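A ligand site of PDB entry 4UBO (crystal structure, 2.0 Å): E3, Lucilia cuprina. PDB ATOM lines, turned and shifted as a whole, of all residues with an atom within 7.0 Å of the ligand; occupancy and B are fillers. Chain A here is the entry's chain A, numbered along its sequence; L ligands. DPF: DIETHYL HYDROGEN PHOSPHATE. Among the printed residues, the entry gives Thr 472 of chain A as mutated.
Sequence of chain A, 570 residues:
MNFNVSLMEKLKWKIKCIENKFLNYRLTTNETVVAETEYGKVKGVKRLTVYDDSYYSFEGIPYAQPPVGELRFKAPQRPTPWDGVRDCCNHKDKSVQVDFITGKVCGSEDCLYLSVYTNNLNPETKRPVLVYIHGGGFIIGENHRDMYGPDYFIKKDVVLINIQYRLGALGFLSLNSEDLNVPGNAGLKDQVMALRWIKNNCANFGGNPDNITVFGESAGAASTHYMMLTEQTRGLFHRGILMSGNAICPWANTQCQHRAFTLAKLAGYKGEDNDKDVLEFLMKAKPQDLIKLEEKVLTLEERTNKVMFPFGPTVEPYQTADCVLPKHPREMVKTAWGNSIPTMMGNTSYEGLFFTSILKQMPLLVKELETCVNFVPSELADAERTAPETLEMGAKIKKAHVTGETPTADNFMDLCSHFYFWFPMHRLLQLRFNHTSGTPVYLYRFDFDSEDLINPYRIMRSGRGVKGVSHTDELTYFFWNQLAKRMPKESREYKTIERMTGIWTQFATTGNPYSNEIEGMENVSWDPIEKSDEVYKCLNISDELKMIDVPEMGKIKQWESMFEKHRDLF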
ATOM      1  N   HIS A 134      16.894 -18.696  18.054  1.00  0.00           N
ATOM      2  CA  HIS A 134      17.141 -19.919  17.294  1.00  0.00           C
ATOM      3  C   HIS A 134      18.592 -20.034  16.795  1.00  0.00           C
ATOM      4  O   HIS A 134      19.263 -19.028  16.619  1.00  0.00           O
ATOM      5  CB  HIS A 134      16.175 -19.995  16.107  1.00  0.00           C
ATOM      6  CG  HIS A 134      16.513 -19.048  14.992  1.00  0.00           C
ATOM      7  ND1 HIS A 134      17.554 -19.276  14.111  1.00  0.00           N
ATOM      8  CD2 HIS A 134      15.946 -17.887  14.612  1.00  0.00           C
ATOM      9  CE1 HIS A 134      17.595 -18.301  13.232  1.00  0.00           C
ATOM     10  NE2 HIS A 134      16.635 -17.447  13.505  1.00  0.00           N
ATOM     11  N   GLY A 135      19.057 -21.269  16.582  1.00  0.00           N
ATOM     12  CA  GLY A 135      20.359 -21.508  16.002  1.00  0.00           C
ATOM     13  C   GLY A 135      20.263 -21.649  14.504  1.00  0.00           C
ATOM     14  O   GLY A 135      19.246 -21.297  13.902  1.00  0.00           O
ATOM     15  N   GLY A 136      21.330 -22.150  13.873  1.00  0.00           N
ATOM     16  CA  GLY A 136      21.372 -22.223  12.435  1.00  0.00           C
ATOM     17  C   GLY A 136      22.613 -21.547  11.884  1.00  0.00           C
ATOM     18  O   GLY A 136      22.592 -20.961  10.801  1.00  0.00           O
ATOM     19  N   GLY A 137      23.699 -21.622  12.651  1.00  0.00           N
ATOM     20  CA  GLY A 137      25.003 -21.123  12.254  1.00  0.00           C
ATOM     21  C   GLY A 137      25.072 -19.650  11.926  1.00  0.00           C
ATOM     22  O   GLY A 137      26.068 -19.192  11.370  1.00  0.00           O
ATOM     23  N   PHE A 138      24.032 -18.908  12.318  1.00  0.00           N
ATOM     24  CA  PHE A 138      23.829 -17.499  11.981  1.00  0.00           C
ATOM     25  C   PHE A 138      23.540 -17.315  10.500  1.00  0.00           C
ATOM     26  O   PHE A 138      23.628 -16.188   9.991  1.00  0.00           O
ATOM     27  CB  PHE A 138      25.031 -16.612  12.353  1.00  0.00           C
ATOM     28  CG  PHE A 138      25.350 -16.586  13.824  1.00  0.00           C
ATOM     29  CD1 PHE A 138      24.629 -15.786  14.688  1.00  0.00           C
ATOM     30  CD2 PHE A 138      26.410 -17.334  14.330  1.00  0.00           C
ATOM     31  CE1 PHE A 138      24.941 -15.735  16.034  1.00  0.00           C
ATOM     32  CE2 PHE A 138      26.722 -17.283  15.676  1.00  0.00           C
ATOM     33  CZ  PHE A 138      25.990 -16.490  16.530  1.00  0.00           C
ATOM     34  N   ILE A 140      20.940 -19.621   8.813  1.00  0.00           N
ATOM     35  CA  ILE A 140      19.583 -20.104   8.559  1.00  0.00           C
ATOM     36  C   ILE A 140      18.720 -19.983   9.823  1.00  0.00           C
ATOM     37  O   ILE A 140      19.241 -19.715  10.911  1.00  0.00           O
ATOM     38  CB  ILE A 140      19.524 -21.587   8.096  1.00  0.00           C
ATOM     39  CG1 ILE A 140      20.079 -22.513   9.193  1.00  0.00           C
ATOM     40  CG2 ILE A 140      20.235 -21.806   6.764  1.00  0.00           C
ATOM     41  CD1 ILE A 140      19.618 -23.906   9.066  1.00  0.00           C
ATOM     42  N   TYR A 165      16.207 -12.506  13.567  1.00  0.00           N
ATOM     43  CA  TYR A 165      17.324 -11.554  13.504  1.00  0.00           C
ATOM     44  C   TYR A 165      18.014 -11.784  12.164  1.00  0.00           C
ATOM     45  O   TYR A 165      17.872 -12.868  11.595  1.00  0.00           O
ATOM     46  CB  TYR A 165      18.272 -11.755  14.681  1.00  0.00           C
ATOM     47  CG  TYR A 165      18.821 -13.176  14.782  1.00  0.00           C
ATOM     48  CD1 TYR A 165      18.128 -14.185  15.448  1.00  0.00           C
ATOM     49  CD2 TYR A 165      20.051 -13.497  14.216  1.00  0.00           C
ATOM     50  CE1 TYR A 165      18.653 -15.464  15.551  1.00  0.00           C
ATOM     51  CE2 TYR A 165      20.560 -14.762  14.308  1.00  0.00           C
ATOM     52  CZ  TYR A 165      19.871 -15.748  14.971  1.00  0.00           C
ATOM     53  OH  TYR A 165      20.424 -17.006  15.038  1.00  0.00           O
ATOM     54  N   GLU A 217      19.868 -22.467  21.262  1.00  0.00           N
ATOM     55  CA  GLU A 217      20.591 -23.689  20.949  1.00  0.00           C
ATOM     56  C   GLU A 217      21.544 -23.419  19.753  1.00  0.00           C
ATOM     57  O   GLU A 217      21.192 -22.690  18.841  1.00  0.00           O
ATOM     58  CB  GLU A 217      19.574 -24.807  20.662  1.00  0.00           C
ATOM     59  CG  GLU A 217      20.131 -26.207  20.563  1.00  0.00           C
ATOM     60  CD  GLU A 217      20.451 -26.585  19.131  1.00  0.00           C
ATOM     61  OE1 GLU A 217      20.005 -25.866  18.216  1.00  0.00           O
ATOM     62  OE2 GLU A 217      21.168 -27.582  18.930  1.00  0.00           O
ATOM     63  N   SER A 218      22.758 -23.982  19.800  1.00  0.00           N
ATOM     64  CA  SER A 218      23.805 -23.798  18.762  1.00  0.00           C
ATOM     65  C   SER A 218      24.242 -22.321  18.589  1.00  0.00           C
ATOM     66  O   SER A 218      24.712 -21.683  19.545  1.00  0.00           O
ATOM     67  CB  SER A 218      23.313 -24.392  17.430  1.00  0.00           C
ATOM     68  OG  SER A 218      24.347 -24.396  16.452  1.00  0.00           O
ATOM     69  N   ALA A 219      24.085 -21.775  17.389  1.00  0.00           N
ATOM     70  CA  ALA A 219      24.243 -20.339  17.162  1.00  0.00           C
ATOM     71  C   ALA A 219      23.303 -19.511  18.026  1.00  0.00           C
ATOM     72  O   ALA A 219      23.575 -18.344  18.273  1.00  0.00           O
ATOM     73  CB  ALA A 219      24.022 -20.009  15.673  1.00  0.00           C
ATOM     74  N   GLY A 220      22.177 -20.085  18.464  1.00  0.00           N
ATOM     75  CA  GLY A 220      21.293 -19.427  19.418  1.00  0.00           C
ATOM     76  C   GLY A 220      21.823 -19.459  20.832  1.00  0.00           C
ATOM     77  O   GLY A 220      21.516 -18.574  21.651  1.00  0.00           O
ATOM     78  N   ALA A 221      22.634 -20.477  21.140  1.00  0.00           N
ATOM     79  CA  ALA A 221      23.345 -20.529  22.410  1.00  0.00           C
ATOM     80  C   ALA A 221      24.463 -19.503  22.424  1.00  0.00           C
ATOM     81  O   ALA A 221      24.644 -18.790  23.404  1.00  0.00           O
ATOM     82  CB  ALA A 221      23.906 -21.937  22.651  1.00  0.00           C
ATOM     83  N   SER A 244      24.181 -26.403  24.024  1.00  0.00           N
ATOM     84  CA  SER A 244      25.131 -26.820  22.978  1.00  0.00           C
ATOM     85  C   SER A 244      25.839 -25.631  22.339  1.00  0.00           C
ATOM     86  O   SER A 244      25.869 -25.527  21.108  1.00  0.00           O
ATOM     87  CB  SER A 244      24.428 -27.636  21.891  1.00  0.00           C
ATOM     88  OG  SER A 244      23.949 -28.879  22.376  1.00  0.00           O
ATOM     89  N   TRP A 251      33.396 -21.680  16.064  1.00  0.00           N
ATOM     90  CA  TRP A 251      32.518 -21.295  14.965  1.00  0.00           C
ATOM     91  C   TRP A 251      31.727 -20.021  15.267  1.00  0.00           C
ATOM     92  O   TRP A 251      31.043 -19.490  14.403  1.00  0.00           O
ATOM     93  CB  TRP A 251      31.520 -22.431  14.652  1.00  0.00           C
ATOM     94  CG  TRP A 251      30.932 -23.011  15.891  1.00  0.00           C
ATOM     95  CD1 TRP A 251      31.399 -24.080  16.589  1.00  0.00           C
ATOM     96  CD2 TRP A 251      29.784 -22.534  16.598  1.00  0.00           C
ATOM     97  NE1 TRP A 251      30.616 -24.318  17.692  1.00  0.00           N
ATOM     98  CE2 TRP A 251      29.604 -23.377  17.723  1.00  0.00           C
ATOM     99  CE3 TRP A 251      28.879 -21.484  16.408  1.00  0.00           C
ATOM    100  CZ2 TRP A 251      28.575 -23.192  18.651  1.00  0.00           C
ATOM    101  CZ3 TRP A 251      27.839 -21.307  17.325  1.00  0.00           C
ATOM    102  CH2 TRP A 251      27.698 -22.158  18.432  1.00  0.00           C
ATOM    103  N   MET A 308      34.124 -22.058   9.607  1.00  0.00           N
ATOM    104  CA  MET A 308      32.880 -22.730   9.240  1.00  0.00           C
ATOM    105  C   MET A 308      31.976 -21.853   8.388  1.00  0.00           C
ATOM    106  O   MET A 308      31.358 -22.320   7.433  1.00  0.00           O
ATOM    107  CB  MET A 308      32.144 -23.213  10.495  1.00  0.00           C
ATOM    108  CG  MET A 308      31.088 -24.280  10.187  1.00  0.00           C
ATOM    109  SD  MET A 308      30.137 -24.830  11.618  1.00  0.00           S
ATOM    110  CE  MET A 308      31.247 -26.007  12.357  1.00  0.00           C
ATOM    111  N   PHE A 309      31.912 -20.563   8.731  1.00  0.00           N
ATOM    112  CA  PHE A 309      31.059 -19.622   8.014  1.00  0.00           C
ATOM    113  C   PHE A 309      31.819 -18.337   7.629  1.00  0.00           C
ATOM    114  O   PHE A 309      32.563 -17.797   8.443  1.00  0.00           O
ATOM    115  CB  PHE A 309      29.849 -19.257   8.868  1.00  0.00           C
ATOM    116  CG  PHE A 309      29.143 -20.450   9.470  1.00  0.00           C
ATOM    117  CD1 PHE A 309      28.351 -21.278   8.686  1.00  0.00           C
ATOM    118  CD2 PHE A 309      29.272 -20.726  10.821  1.00  0.00           C
ATOM    119  CE1 PHE A 309      27.679 -22.370   9.227  1.00  0.00           C
ATOM    120  CE2 PHE A 309      28.583 -21.818  11.380  1.00  0.00           C
ATOM    121  CZ  PHE A 309      27.795 -22.645  10.572  1.00  0.00           C
ATOM    122  N   PHE A 354      26.290 -35.479  14.603  1.00  0.00           N
ATOM    123  CA  PHE A 354      25.737 -34.602  13.587  1.00  0.00           C
ATOM    124  C   PHE A 354      26.505 -34.618  12.265  1.00  0.00           C
ATOM    125  O   PHE A 354      25.926 -34.421  11.193  1.00  0.00           O
ATOM    126  CB  PHE A 354      25.688 -33.183  14.153  1.00  0.00           C
ATOM    127  CG  PHE A 354      25.057 -32.187  13.241  1.00  0.00           C
ATOM    128  CD1 PHE A 354      25.826 -31.469  12.341  1.00  0.00           C
ATOM    129  CD2 PHE A 354      23.688 -31.976  13.281  1.00  0.00           C
ATOM    130  CE1 PHE A 354      25.242 -30.553  11.492  1.00  0.00           C
ATOM    131  CE2 PHE A 354      23.100 -31.057  12.424  1.00  0.00           C
ATOM    132  CZ  PHE A 354      23.875 -30.346  11.541  1.00  0.00           C
ATOM    133  N   PHE A 355      27.813 -34.826  12.318  1.00  0.00           N
ATOM    134  CA  PHE A 355      28.673 -34.625  11.148  1.00  0.00           C
ATOM    135  C   PHE A 355      28.743 -35.801  10.197  1.00  0.00           C
ATOM    136  O   PHE A 355      29.590 -35.814   9.307  1.00  0.00           O
ATOM    137  CB  PHE A 355      30.098 -34.295  11.599  1.00  0.00           C
ATOM    138  CG  PHE A 355      30.237 -32.907  12.117  1.00  0.00           C
ATOM    139  CD1 PHE A 355      30.245 -31.830  11.249  1.00  0.00           C
ATOM    140  CD2 PHE A 355      30.325 -32.668  13.477  1.00  0.00           C
ATOM    141  CE1 PHE A 355      30.355 -30.547  11.720  1.00  0.00           C
ATOM    142  CE2 PHE A 355      30.433 -31.367  13.957  1.00  0.00           C
ATOM    143  CZ  PHE A 355      30.450 -30.310  13.065  1.00  0.00           C
ATOM    144  N   TYR A 420      34.048 -28.646  18.880  1.00  0.00           N
ATOM    145  CA  TYR A 420      33.017 -27.660  18.673  1.00  0.00           C
ATOM    146  C   TYR A 420      32.241 -27.300  19.930  1.00  0.00           C
ATOM    147  O   TYR A 420      31.728 -26.183  20.005  1.00  0.00           O
ATOM    148  CB  TYR A 420      32.047 -28.137  17.578  1.00  0.00           C
ATOM    149  CG  TYR A 420      32.703 -28.214  16.213  1.00  0.00           C
ATOM    150  CD1 TYR A 420      33.101 -27.057  15.536  1.00  0.00           C
ATOM    151  CD2 TYR A 420      32.912 -29.441  15.591  1.00  0.00           C
ATOM    152  CE1 TYR A 420      33.718 -27.138  14.263  1.00  0.00           C
ATOM    153  CE2 TYR A 420      33.509 -29.532  14.356  1.00  0.00           C
ATOM    154  CZ  TYR A 420      33.910 -28.378  13.687  1.00  0.00           C
ATOM    155  OH  TYR A 420      34.506 -28.511  12.446  1.00  0.00           O
ATOM    156  N   PHE A 421      32.145 -28.191  20.923  1.00  0.00           N
ATOM    157  CA  PHE A 421      31.208 -27.965  22.042  1.00  0.00           C
ATOM    158  C   PHE A 421      31.786 -28.124  23.476  1.00  0.00           C
ATOM    159  O   PHE A 421      31.731 -27.171  24.267  1.00  0.00           O
ATOM    160  CB  PHE A 421      29.986 -28.870  21.865  1.00  0.00           C
ATOM    161  CG  PHE A 421      29.286 -28.682  20.524  1.00  0.00           C
ATOM    162  CD1 PHE A 421      28.508 -27.549  20.288  1.00  0.00           C
ATOM    163  CD2 PHE A 421      29.407 -29.619  19.508  1.00  0.00           C
ATOM    164  CE1 PHE A 421      27.888 -27.350  19.061  1.00  0.00           C
ATOM    165  CE2 PHE A 421      28.789 -29.437  18.272  1.00  0.00           C
ATOM    166  CZ  PHE A 421      28.035 -28.299  18.054  1.00  0.00           C
ATOM    167  N   TYR A 457      16.099 -31.150  11.583  1.00  0.00           N
ATOM    168  CA  TYR A 457      17.557 -31.243  11.504  1.00  0.00           C
ATOM    169  C   TYR A 457      18.037 -32.668  11.250  1.00  0.00           C
ATOM    170  O   TYR A 457      19.145 -32.886  10.762  1.00  0.00           O
ATOM    171  CB  TYR A 457      18.212 -30.723  12.779  1.00  0.00           C
ATOM    172  CG  TYR A 457      18.312 -29.223  12.843  1.00  0.00           C
ATOM    173  CD1 TYR A 457      19.296 -28.542  12.124  1.00  0.00           C
ATOM    174  CD2 TYR A 457      17.447 -28.473  13.635  1.00  0.00           C
ATOM    175  CE1 TYR A 457      19.403 -27.169  12.176  1.00  0.00           C
ATOM    176  CE2 TYR A 457      17.547 -27.097  13.702  1.00  0.00           C
ATOM    177  CZ  TYR A 457      18.526 -26.454  12.968  1.00  0.00           C
ATOM    178  OH  TYR A 457      18.646 -25.083  13.027  1.00  0.00           O
ATOM    179  N   MET A 460      18.598 -32.952   7.620  1.00  0.00           N
ATOM    180  CA  MET A 460      19.824 -32.279   7.213  1.00  0.00           C
ATOM    181  C   MET A 460      21.061 -33.135   7.481  1.00  0.00           C
ATOM    182  O   MET A 460      21.862 -33.367   6.570  1.00  0.00           O
ATOM    183  CB  MET A 460      19.938 -30.934   7.928  1.00  0.00           C
ATOM    184  CG  MET A 460      21.141 -30.114   7.535  1.00  0.00           C
ATOM    185  SD  MET A 460      21.340 -28.631   8.544  1.00  0.00           S
ATOM    186  CE  MET A 460      19.803 -27.772   8.191  1.00  0.00           C
ATOM    187  N   HIS A 471      23.626 -33.414  18.302  1.00  0.00           N
ATOM    188  CA  HIS A 471      23.345 -31.987  18.301  1.00  0.00           C
ATOM    189  C   HIS A 471      21.981 -31.744  17.651  1.00  0.00           C
ATOM    190  O   HIS A 471      21.695 -32.323  16.596  1.00  0.00           O
ATOM    191  CB  HIS A 471      24.488 -31.257  17.546  1.00  0.00           C
ATOM    192  CG  HIS A 471      24.375 -29.768  17.556  1.00  0.00           C
ATOM    193  ND1 HIS A 471      24.624 -29.006  18.682  1.00  0.00           N
ATOM    194  CD2 HIS A 471      24.052 -28.890  16.572  1.00  0.00           C
ATOM    195  CE1 HIS A 471      24.450 -27.723  18.383  1.00  0.00           C
ATOM    196  NE2 HIS A 471      24.102 -27.635  17.111  1.00  0.00           N
ATOM    197  N   THR A 472      21.138 -30.925  18.304  1.00  0.00           N
ATOM    198  CA  THR A 472      19.752 -30.572  17.883  1.00  0.00           C
ATOM    199  C   THR A 472      18.662 -31.608  18.175  1.00  0.00           C
ATOM    200  O   THR A 472      17.488 -31.308  17.988  1.00  0.00           O
ATOM    201  CB  THR A 472      19.585 -30.283  16.356  1.00  0.00           C
ATOM    202  OG1 THR A 472      19.591 -31.529  15.628  1.00  0.00           O
ATOM    203  CG2 THR A 472      20.661 -29.348  15.829  1.00  0.00           C
ATOM    204  N   LEU A 475      15.772 -30.463  20.684  1.00  0.00           N
ATOM    205  CA  LEU A 475      14.782 -29.472  20.269  1.00  0.00           C
ATOM    206  C   LEU A 475      13.403 -30.108  20.117  1.00  0.00           C
ATOM    207  O   LEU A 475      12.381 -29.436  20.219  1.00  0.00           O
ATOM    208  CB  LEU A 475      15.185 -28.823  18.955  1.00  0.00           C
ATOM    209  CG  LEU A 475      16.406 -27.914  19.008  1.00  0.00           C
ATOM    210  CD1 LEU A 475      16.693 -27.313  17.646  1.00  0.00           C
ATOM    211  CD2 LEU A 475      16.194 -26.820  20.067  1.00  0.00           C
HETATM  212  O4  DPF L   1      23.635 -23.173  15.070  1.00  0.00           O
HETATM  213  P1  DPF L   1      24.158 -24.583  14.956  1.00  0.00           P
HETATM  214  O3  DPF L   1      25.672 -24.433  14.296  1.00  0.00           O
HETATM  215  C1  DPF L   1      26.759 -24.287  15.112  1.00  0.00           C
HETATM  216  C4  DPF L   1      27.914 -25.020  14.475  1.00  0.00           C
HETATM  217  O1  DPF L   1      23.307 -25.206  13.685  1.00  0.00           O
HETATM  218  C2  DPF L   1      22.239 -26.016  13.953  1.00  0.00           C
HETATM  219  C3  DPF L   1      22.691 -27.439  13.756  1.00  0.00           C
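The backbone NH (N) of Gly 137 sits at hydrogen-bond distance from an oxygen (O4) of the ligand, at 2.9 Å. N of Ala 219 sits at hydrogen-bond distance from O4 of the ligand, 2.7 Å away. The side-chain hydroxyl (OG) of Ser 218 is covalently linked to a phosphorus (P1) of the ligand, 1.5 Å away. N of Gly 136 lies within hydrogen-bond range of O4 of the ligand.
The backbone NH of Thr 472 sits at hydrogen-bond distance from the side-chain carboxylate of Glu 217 (3.4 Å). The backbone NH of Gly 135 lies close to the backbone carbonyl oxygen of Glu 217, 3.4 Å away. OG of Ser 218 sits at hydrogen-bond distance from NE2 of His 471, at 3.3 Å. NE1 of Trp 251 lies within hydrogen-bond range of O of Tyr 420 (3.2 Å). The side-chain carboxylate of Glu 217 sits close to a ring nitrogen (NE2) of His 471 (3.5 Å).
Residues that only touch the ligand: His 471 (3.4 Å), Thr 472 (3.5 Å), Tyr 457 (3.5 Å), Met 308 (3.6 Å), Gly 135 (3.7 Å), Trp 251 (3.7 Å) and Phe 354 (3.8 Å). Hydrophobic or aromatic side chains that line the ligand: Ala 219, Trp 251, Met 308, Phe 354, Tyr 457 and His 471. 11 residues have an atom within 4 Å of the ligand: Gly 135, Gly 136, Gly 137, Ser 218, Ala 219, Trp 251, Met 308, Phe 354, Tyr 457, His 471 and Thr 472. The nearest printed residue that does not touch the ligand is Phe 309 (4.5 Å).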
